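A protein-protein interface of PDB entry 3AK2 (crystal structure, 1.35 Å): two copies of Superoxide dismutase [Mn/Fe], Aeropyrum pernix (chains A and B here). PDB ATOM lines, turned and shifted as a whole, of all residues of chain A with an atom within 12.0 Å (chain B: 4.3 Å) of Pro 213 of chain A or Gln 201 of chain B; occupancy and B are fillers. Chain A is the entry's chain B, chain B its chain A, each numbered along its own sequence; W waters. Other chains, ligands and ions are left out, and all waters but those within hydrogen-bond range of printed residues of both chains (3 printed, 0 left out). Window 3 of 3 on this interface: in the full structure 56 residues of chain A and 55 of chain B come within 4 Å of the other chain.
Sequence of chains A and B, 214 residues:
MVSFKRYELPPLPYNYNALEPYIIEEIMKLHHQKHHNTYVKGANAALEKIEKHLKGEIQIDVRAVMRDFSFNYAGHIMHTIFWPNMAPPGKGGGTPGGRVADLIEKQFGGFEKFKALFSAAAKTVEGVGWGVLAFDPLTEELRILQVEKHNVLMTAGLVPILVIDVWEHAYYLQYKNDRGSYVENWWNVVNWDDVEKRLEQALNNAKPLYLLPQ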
ATOM      1  N   PRO A 137      13.546  -6.140 -35.260  1.00  0.00           N
ATOM      2  CA  PRO A 137      13.531  -6.677 -33.898  1.00  0.00           C
ATOM      3  C   PRO A 137      12.127  -6.899 -33.334  1.00  0.00           C
ATOM      4  O   PRO A 137      11.968  -7.685 -32.401  1.00  0.00           O
ATOM      5  CB  PRO A 137      14.256  -5.598 -33.090  1.00  0.00           C
ATOM      6  CG  PRO A 137      14.048  -4.343 -33.871  1.00  0.00           C
ATOM      7  CD  PRO A 137      14.113  -4.779 -35.304  1.00  0.00           C
ATOM      8  N   LEU A 138      11.127  -6.217 -33.890  1.00  0.00           N
ATOM      9  CA  LEU A 138       9.764  -6.303 -33.371  1.00  0.00           C
ATOM     10  C   LEU A 138       9.035  -7.580 -33.795  1.00  0.00           C
ATOM     11  O   LEU A 138       8.129  -8.036 -33.095  1.00  0.00           O
ATOM     12  CB  LEU A 138       8.949  -5.064 -33.766  1.00  0.00           C
ATOM     13  CG  LEU A 138       9.466  -3.690 -33.314  1.00  0.00           C
ATOM     14  CD1 LEU A 138       8.468  -2.607 -33.697  1.00  0.00           C
ATOM     15  CD2 LEU A 138       9.753  -3.633 -31.813  1.00  0.00           C
ATOM     16  N   GLU A 140      11.023 -10.199 -35.631  1.00  0.00           N
ATOM     17  CA  GLU A 140      12.085 -11.148 -35.986  1.00  0.00           C
ATOM     18  C   GLU A 140      11.950 -11.656 -37.429  1.00  0.00           C
ATOM     19  O   GLU A 140      12.161 -12.836 -37.725  1.00  0.00           O
ATOM     20  CB  GLU A 140      12.205 -12.276 -34.946  1.00  0.00           C
ATOM     21  CG  GLU A 140      12.650 -11.764 -33.572  1.00  0.00           C
ATOM     22  CD  GLU A 140      13.086 -12.863 -32.622  1.00  0.00           C
ATOM     23  OE1 GLU A 140      14.233 -12.806 -32.131  1.00  0.00           O
ATOM     24  OE2 GLU A 140      12.280 -13.779 -32.358  1.00  0.00           O
ATOM     25  N   VAL A 159      17.789  -3.650 -38.243  1.00  0.00           N
ATOM     26  CA  VAL A 159      19.223  -3.925 -38.267  1.00  0.00           C
ATOM     27  C   VAL A 159      19.623  -4.330 -39.684  1.00  0.00           C
ATOM     28  O   VAL A 159      19.223  -5.402 -40.146  1.00  0.00           O
ATOM     29  CB  VAL A 159      19.587  -5.071 -37.283  1.00  0.00           C
ATOM     30  CG1 VAL A 159      21.086  -5.359 -37.316  1.00  0.00           C
ATOM     31  CG2 VAL A 159      19.141  -4.742 -35.867  1.00  0.00           C
ATOM     32  N   GLN A 201      23.540 -13.107 -35.324  1.00  0.00           N
ATOM     33  CA  GLN A 201      23.657 -12.136 -34.240  1.00  0.00           C
ATOM     34  C   GLN A 201      22.336 -11.412 -33.981  1.00  0.00           C
ATOM     35  O   GLN A 201      21.941 -11.227 -32.830  1.00  0.00           O
ATOM     36  CB  GLN A 201      24.789 -11.135 -34.505  1.00  0.00           C
ATOM     37  CG  GLN A 201      26.187 -11.764 -34.546  1.00  0.00           C
ATOM     38  CD  GLN A 201      26.527 -12.572 -33.298  1.00  0.00           C
ATOM     39  OE1 GLN A 201      26.982 -13.712 -33.396  1.00  0.00           O
ATOM     40  NE2 GLN A 201      26.307 -11.985 -32.123  1.00  0.00           N
ATOM     41  N   ALA A 202      21.643 -11.038 -35.054  1.00  0.00           N
ATOM     42  CA  ALA A 202      20.361 -10.344 -34.931  1.00  0.00           C
ATOM     43  C   ALA A 202      19.292 -11.207 -34.256  1.00  0.00           C
ATOM     44  O   ALA A 202      18.555 -10.731 -33.390  1.00  0.00           O
ATOM     45  CB  ALA A 202      19.889  -9.847 -36.290  1.00  0.00           C
ATOM     46  N   LEU A 203      19.234 -12.481 -34.635  1.00  0.00           N
ATOM     47  CA  LEU A 203      18.304 -13.431 -34.022  1.00  0.00           C
ATOM     48  C   LEU A 203      18.529 -13.580 -32.514  1.00  0.00           C
ATOM     49  O   LEU A 203      17.574 -13.722 -31.748  1.00  0.00           O
ATOM     50  CB  LEU A 203      18.391 -14.794 -34.717  1.00  0.00           C
ATOM     51  CG  LEU A 203      17.718 -14.894 -36.089  1.00  0.00           C
ATOM     52  CD1 LEU A 203      18.271 -16.068 -36.872  1.00  0.00           C
ATOM     53  CD2 LEU A 203      16.200 -14.999 -35.964  1.00  0.00           C
ATOM     54  N   ASN A 204      19.792 -13.535 -32.096  1.00  0.00           N
ATOM     55  CA  ASN A 204      20.145 -13.656 -30.686  1.00  0.00           C
ATOM     56  C   ASN A 204      19.981 -12.359 -29.892  1.00  0.00           C
ATOM     57  O   ASN A 204      19.604 -12.397 -28.717  1.00  0.00           O
ATOM     58  CB  ASN A 204      21.582 -14.172 -30.533  1.00  0.00           C
ATOM     59  CG  ASN A 204      21.742 -15.616 -30.977  1.00  0.00           C
ATOM     60  OD1 ASN A 204      20.782 -16.387 -31.003  1.00  0.00           O
ATOM     61  ND2 ASN A 204      22.970 -15.993 -31.319  1.00  0.00           N
ATOM     62  N   ASN A 205      20.254 -11.224 -30.536  1.00  0.00           N
ATOM     63  CA  ASN A 205      20.472  -9.955 -29.827  1.00  0.00           C
ATOM     64  C   ASN A 205      19.514  -8.787 -30.088  1.00  0.00           C
ATOM     65  O   ASN A 205      19.391  -7.907 -29.237  1.00  0.00           O
ATOM     66  CB  ASN A 205      21.910  -9.471 -30.052  1.00  0.00           C
ATOM     67  CG  ASN A 205      22.934 -10.294 -29.290  1.00  0.00           C
ATOM     68  OD1 ASN A 205      22.682 -11.440 -28.914  1.00  0.00           O
ATOM     69  ND2 ASN A 205      24.098  -9.709 -29.058  1.00  0.00           N
ATOM     70  N   ALA A 206      18.851  -8.765 -31.242  1.00  0.00           N
ATOM     71  CA  ALA A 206      18.105  -7.567 -31.664  1.00  0.00           C
ATOM     72  C   ALA A 206      16.832  -7.278 -30.862  1.00  0.00           C
ATOM     73  O   ALA A 206      16.633  -6.163 -30.382  1.00  0.00           O
ATOM     74  CB  ALA A 206      17.806  -7.613 -33.159  1.00  0.00           C
ATOM     75  N   LYS A 207      15.971  -8.281 -30.719  1.00  0.00           N
ATOM     76  CA  LYS A 207      14.678  -8.087 -30.056  1.00  0.00           C
ATOM     77  C   LYS A 207      14.754  -7.441 -28.649  1.00  0.00           C
ATOM     78  O   LYS A 207      14.049  -6.458 -28.396  1.00  0.00           O
ATOM     79  CB  LYS A 207      13.895  -9.404 -30.041  1.00  0.00           C
ATOM     80  CG  LYS A 207      12.490  -9.321 -29.478  1.00  0.00           C
ATOM     81  CD  LYS A 207      11.778 -10.641 -29.706  1.00  0.00           C
ATOM     82  CE  LYS A 207      10.482 -10.733 -28.933  1.00  0.00           C
ATOM     83  NZ  LYS A 207       9.776 -11.996 -29.283  1.00  0.00           N
ATOM     84  N   PRO A 208      15.613  -7.970 -27.746  1.00  0.00           N
ATOM     85  CA  PRO A 208      15.741  -7.417 -26.383  1.00  0.00           C
ATOM     86  C   PRO A 208      16.109  -5.927 -26.261  1.00  0.00           C
ATOM     87  O   PRO A 208      15.906  -5.340 -25.196  1.00  0.00           O
ATOM     88  CB  PRO A 208      16.855  -8.269 -25.766  1.00  0.00           C
ATOM     89  CG  PRO A 208      16.835  -9.528 -26.517  1.00  0.00           C
ATOM     90  CD  PRO A 208      16.490  -9.143 -27.922  1.00  0.00           C
ATOM     91  N   LEU A 209      16.645  -5.324 -27.321  1.00  0.00           N
ATOM     92  CA  LEU A 209      17.008  -3.903 -27.298  1.00  0.00           C
ATOM     93  C   LEU A 209      15.789  -2.996 -27.159  1.00  0.00           C
ATOM     94  O   LEU A 209      15.905  -1.851 -26.710  1.00  0.00           O
ATOM     95  CB  LEU A 209      17.757  -3.514 -28.576  1.00  0.00           C
ATOM     96  CG  LEU A 209      19.148  -4.083 -28.854  1.00  0.00           C
ATOM     97  CD1 LEU A 209      19.587  -3.724 -30.266  1.00  0.00           C
ATOM     98  CD2 LEU A 209      20.150  -3.573 -27.832  1.00  0.00           C
ATOM     99  N   TYR A 210      14.628  -3.526 -27.540  1.00  0.00           N
ATOM    100  CA  TYR A 210      13.418  -2.725 -27.704  1.00  0.00           C
ATOM    101  C   TYR A 210      12.248  -3.248 -26.894  1.00  0.00           C
ATOM    102  O   TYR A 210      11.536  -2.477 -26.245  1.00  0.00           O
ATOM    103  CB  TYR A 210      13.065  -2.657 -29.187  1.00  0.00           C
ATOM    104  CG  TYR A 210      14.160  -1.996 -29.968  1.00  0.00           C
ATOM    105  CD1 TYR A 210      14.354  -0.625 -29.870  1.00  0.00           C
ATOM    106  CD2 TYR A 210      15.032  -2.737 -30.766  1.00  0.00           C
ATOM    107  CE1 TYR A 210      15.357   0.003 -30.554  1.00  0.00           C
ATOM    108  CE2 TYR A 210      16.057  -2.111 -31.469  1.00  0.00           C
ATOM    109  CZ  TYR A 210      16.207  -0.733 -31.352  1.00  0.00           C
ATOM    110  OH  TYR A 210      17.195  -0.052 -32.021  1.00  0.00           O
ATOM    111  N   LEU A 211      12.048  -4.559 -26.957  1.00  0.00           N
ATOM    112  CA  LEU A 211      11.059  -5.230 -26.138  1.00  0.00           C
ATOM    113  C   LEU A 211      11.830  -5.927 -25.024  1.00  0.00           C
ATOM    114  O   LEU A 211      12.415  -6.993 -25.231  1.00  0.00           O
ATOM    115  CB  LEU A 211      10.241  -6.216 -26.981  1.00  0.00           C
ATOM    116  CG  LEU A 211       9.655  -5.684 -28.300  1.00  0.00           C
ATOM    117  CD1 LEU A 211       9.014  -6.807 -29.103  1.00  0.00           C
ATOM    118  CD2 LEU A 211       8.659  -4.547 -28.067  1.00  0.00           C
ATOM    119  N   LEU A 212      11.845  -5.293 -23.853  1.00  0.00           N
ATOM    120  CA  LEU A 212      12.676  -5.727 -22.726  1.00  0.00           C
ATOM    121  C   LEU A 212      12.334  -7.137 -22.239  1.00  0.00           C
ATOM    122  O   LEU A 212      11.157  -7.500 -22.178  1.00  0.00           O
ATOM    123  CB  LEU A 212      12.581  -4.727 -21.564  1.00  0.00           C
ATOM    124  CG  LEU A 212      13.037  -3.276 -21.775  1.00  0.00           C
ATOM    125  CD1 LEU A 212      12.717  -2.442 -20.546  1.00  0.00           C
ATOM    126  CD2 LEU A 212      14.523  -3.181 -22.107  1.00  0.00           C
ATOM    127  N   PRO A 213      13.365  -7.938 -21.902  1.00  0.00           N
ATOM    128  CA  PRO A 213      13.150  -9.290 -21.394  1.00  0.00           C
ATOM    129  C   PRO A 213      12.934  -9.314 -19.882  1.00  0.00           C
ATOM    130  O   PRO A 213      12.135  -8.536 -19.359  1.00  0.00           O
ATOM    131  CB  PRO A 213      14.450 -10.007 -21.757  1.00  0.00           C
ATOM    132  CG  PRO A 213      15.493  -8.929 -21.773  1.00  0.00           C
ATOM    133  CD  PRO A 213      14.802  -7.607 -21.993  1.00  0.00           C
ATOM    134  N   LYS B 197      17.284   0.290 -18.050  1.00  0.00           N
ATOM    135  CA  LYS B 197      17.063  -1.060 -18.559  1.00  0.00           C
ATOM    136  C   LYS B 197      17.377  -1.172 -20.053  1.00  0.00           C
ATOM    137  O   LYS B 197      17.942  -2.173 -20.498  1.00  0.00           O
ATOM    138  CB  LYS B 197      15.641  -1.529 -18.255  1.00  0.00           C
ATOM    139  CG  LYS B 197      15.441  -1.913 -16.799  1.00  0.00           C
ATOM    140  CD  LYS B 197      13.986  -2.242 -16.506  1.00  0.00           C
ATOM    141  CE  LYS B 197      13.825  -2.909 -15.145  1.00  0.00           C
ATOM    142  NZ  LYS B 197      14.407  -2.112 -14.025  1.00  0.00           N
ATOM    143  N   ARG B 198      17.035  -0.132 -20.814  1.00  0.00           N
ATOM    144  CA  ARG B 198      17.370  -0.082 -22.240  1.00  0.00           C
ATOM    145  C   ARG B 198      18.878  -0.023 -22.467  1.00  0.00           C
ATOM    146  O   ARG B 198      19.415  -0.752 -23.306  1.00  0.00           O
ATOM    147  CB  ARG B 198      16.660   1.086 -22.927  1.00  0.00           C
ATOM    148  CG  ARG B 198      15.177   0.840 -23.042  1.00  0.00           C
ATOM    149  CD  ARG B 198      14.404   1.975 -23.697  1.00  0.00           C
ATOM    150  NE  ARG B 198      12.981   1.696 -23.538  1.00  0.00           N
ATOM    151  CZ  ARG B 198      12.267   0.900 -24.328  1.00  0.00           C
ATOM    152  NH1 ARG B 198      12.817   0.323 -25.390  1.00  0.00           N
ATOM    153  NH2 ARG B 198      10.987   0.691 -24.055  1.00  0.00           N
ATOM    154  N   LEU B 199      19.562   0.818 -21.696  1.00  0.00           N
ATOM    155  CA  LEU B 199      21.015   0.895 -21.779  1.00  0.00           C
ATOM    156  C   LEU B 199      21.675  -0.441 -21.428  1.00  0.00           C
ATOM    157  O   LEU B 199      22.619  -0.863 -22.094  1.00  0.00           O
ATOM    158  CB  LEU B 199      21.550   2.022 -20.898  1.00  0.00           C
ATOM    159  CG  LEU B 199      23.073   2.194 -20.886  1.00  0.00           C
ATOM    160  CD1 LEU B 199      23.633   2.411 -22.285  1.00  0.00           C
ATOM    161  CD2 LEU B 199      23.474   3.332 -19.983  1.00  0.00           C
ATOM    162  N   GLU B 200      21.166  -1.102 -20.393  1.00  0.00           N
ATOM    163  CA  GLU B 200      21.658  -2.425 -20.016  1.00  0.00           C
ATOM    164  C   GLU B 200      21.571  -3.395 -21.195  1.00  0.00           C
ATOM    165  O   GLU B 200      22.542  -4.085 -21.515  1.00  0.00           O
ATOM    166  CB  GLU B 200      20.877  -2.967 -18.818  1.00  0.00           C
ATOM    167  CG  GLU B 200      21.355  -4.331 -18.333  1.00  0.00           C
ATOM    168  CD  GLU B 200      20.305  -5.086 -17.538  1.00  0.00           C
ATOM    169  OE1 GLU B 200      20.534  -6.280 -17.264  1.00  0.00           O
ATOM    170  OE2 GLU B 200      19.256  -4.500 -17.188  1.00  0.00           O
ATOM    171  N   GLN B 201      20.414  -3.436 -21.852  1.00  0.00           N
ATOM    172  CA  GLN B 201      20.240  -4.305 -23.010  1.00  0.00           C
ATOM    173  C   GLN B 201      21.197  -3.944 -24.144  1.00  0.00           C
ATOM    174  O   GLN B 201      21.785  -4.829 -24.759  1.00  0.00           O
ATOM    175  CB  GLN B 201      18.788  -4.299 -23.498  1.00  0.00           C
ATOM    176  CG  GLN B 201      17.806  -4.950 -22.525  1.00  0.00           C
ATOM    177  CD  GLN B 201      18.225  -6.348 -22.095  1.00  0.00           C
ATOM    178  OE1 GLN B 201      18.493  -7.221 -22.926  1.00  0.00           O
ATOM    179  NE2 GLN B 201      18.281  -6.565 -20.787  1.00  0.00           N
ATOM    180  N   ALA B 202      21.365  -2.647 -24.395  1.00  0.00           N
ATOM    181  CA  ALA B 202      22.280  -2.171 -25.436  1.00  0.00           C
ATOM    182  C   ALA B 202      23.742  -2.517 -25.144  1.00  0.00           C
ATOM    183  O   ALA B 202      24.465  -2.973 -26.032  1.00  0.00           O
ATOM    184  CB  ALA B 202      22.103  -0.677 -25.655  1.00  0.00           C
ATOM    185  N   LEU B 203      24.166  -2.315 -23.898  1.00  0.00           N
ATOM    186  CA  LEU B 203      25.522  -2.674 -23.475  1.00  0.00           C
ATOM    187  C   LEU B 203      25.804  -4.160 -23.690  1.00  0.00           C
ATOM    188  O   LEU B 203      26.920  -4.539 -24.050  1.00  0.00           O
ATOM    189  CB  LEU B 203      25.757  -2.298 -22.010  1.00  0.00           C
ATOM    190  CG  LEU B 203      25.979  -0.818 -21.682  1.00  0.00           C
ATOM    191  CD1 LEU B 203      25.640  -0.541 -20.226  1.00  0.00           C
ATOM    192  CD2 LEU B 203      27.403  -0.379 -21.999  1.00  0.00           C
ATOM    193  N   ASN B 204      24.779  -4.985 -23.484  1.00  0.00           N
ATOM    194  CA  ASN B 204      24.892  -6.437 -23.624  1.00  0.00           C
ATOM    195  C   ASN B 204      24.772  -6.940 -25.063  1.00  0.00           C
ATOM    196  O   ASN B 204      25.380  -7.956 -25.410  1.00  0.00           O
ATOM    197  CB  ASN B 204      23.829  -7.145 -22.767  1.00  0.00           C
ATOM    198  CG  ASN B 204      24.070  -7.004 -21.265  1.00  0.00           C
ATOM    199  OD1 ASN B 204      23.172  -7.270 -20.462  1.00  0.00           O
ATOM    200  ND2 ASN B 204      25.274  -6.595 -20.883  1.00  0.00           N
ATOM    201  N   ASN B 205      24.001  -6.231 -25.891  1.00  0.00           N
ATOM    202  CA  ASN B 205      23.522  -6.777 -27.171  1.00  0.00           C
ATOM    203  C   ASN B 205      23.943  -6.070 -28.472  1.00  0.00           C
ATOM    204  O   ASN B 205      24.018  -6.712 -29.519  1.00  0.00           O
ATOM    205  CB  ASN B 205      21.985  -6.877 -27.158  1.00  0.00           C
ATOM    206  CG  ASN B 205      21.462  -7.929 -26.189  1.00  0.00           C
ATOM    207  OD1 ASN B 205      20.902  -7.601 -25.141  1.00  0.00           O
ATOM    208  ND2 ASN B 205      21.623  -9.197 -26.546  1.00  0.00           N
HETATM  209  O   HOH W   1      15.211   0.823 -26.797  1.00  0.00           O
HETATM  210  O   HOH W   2      20.221 -11.458 -25.768  1.00  0.00           O
HETATM  211  O   HOH W   3      18.319  -0.897 -25.910  1.00  0.00           O
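Printed residues of chain A that touch a printed residue of chain B: Asn 205, Pro 208, Leu 209, Tyr 210, Leu 212 and Pro 213. Hydrophobic or aromatic side chains of chain A within 4 Å of the printed part of chain B: Pro 208, Leu 209, Leu 212 and Pro 213. Of the 9 printed residues of chain B, 5 touch a printed residue of chain A.
Asn 205 of chain B touches its own counterpart, Asn 205 of chain A. Positions printed for both chains: 201, 202, 203, 204 and 205. Of the 9 pairs that touch across the chains among the printed residues, 1 has its exchanged pair printed and touching as well.
Water W3 bridges the backbone carbonyl oxygen (O) of Leu 209 of chain A (2.7 Å) and the backbone carbonyl oxygen (O) of Arg 198 of chain B (2.8 Å). Water W1 lies within hydrogen-bond range of O of Leu 209 of chain A and NH1 of Arg 198 of chain B. Water W2 bridges the side-chain amide nitrogen of Asn 205 of chain B (2.8 Å) and the backbone carbonyl oxygen of Asn 204 of chain A (3.2 Å).
Among the printed residues, merely in contact across the chains: Pro 208 of chain A with Gln 201 of chain B (3.3 Å), Leu 209 of chain A with Gln 201 of chain B (3.7 Å), Leu 209 of chain A with Ala 202 of chain B (3.5 Å), Leu 209 of chain A with Asn 205 of chain B (3.8 Å), Leu 212 of chain A with Lys 197 of chain B (3.8 Å), Leu 212 of chain A with Gln 201 of chain B (3.8 Å) and Pro 213 of chain A with Gln 201 of chain B (3.6 Å).
Of chain B, only Gln 201 (3.6 Å) comes within 4 Å of Pro 213 of chain A. Gln 201 of chain B touches just these residues of chain A: Pro 208 (3.3 Å), Leu 209 (3.7 Å), Leu 212 (3.8 Å) and Pro 213 (3.6 Å). No residue of chain A comes within 4 Å of Leu 199 of chain B. No residue of chain A comes within 4 Å of Glu 200 of chain B. Ala 202 of chain B touches one residue of chain A. No residue of chain A comes within 4 Å of Leu 203 of chain B. No residue of chain A comes within 4 Å of Asn 204 of chain B. Of chain A, only Asn 205 and Leu 209 come within 4 Å of Asn 205 of chain B. Of the printed residues of chain B, Asn 205 of chain A touches Asn 205 (3.0 Å). Of the printed residues of chain A, Arg 198 of chain B touches Tyr 210 (3.2 Å). Printed residues of chain B within 4 Å of Tyr 210 of chain A: Arg 198 (3.2 Å). Pro 137 of chain A touches none of the printed residues of chain B.
The backbone carbonyl oxygen (O) of Gln 201 of chain B lies close to the side-chain amide oxygen (OD1) of Asn 205 of chain B.
The guanidinium group (NH1) of Arg 198 of chain B sits at hydrogen-bond distance from the backbone carbonyl oxygen (O) of Tyr 210 of chain A. ND2 of Asn 205 of chain A is in hydrogen-bond range of O of Asn 205 of chain B, at 3.0 Å.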
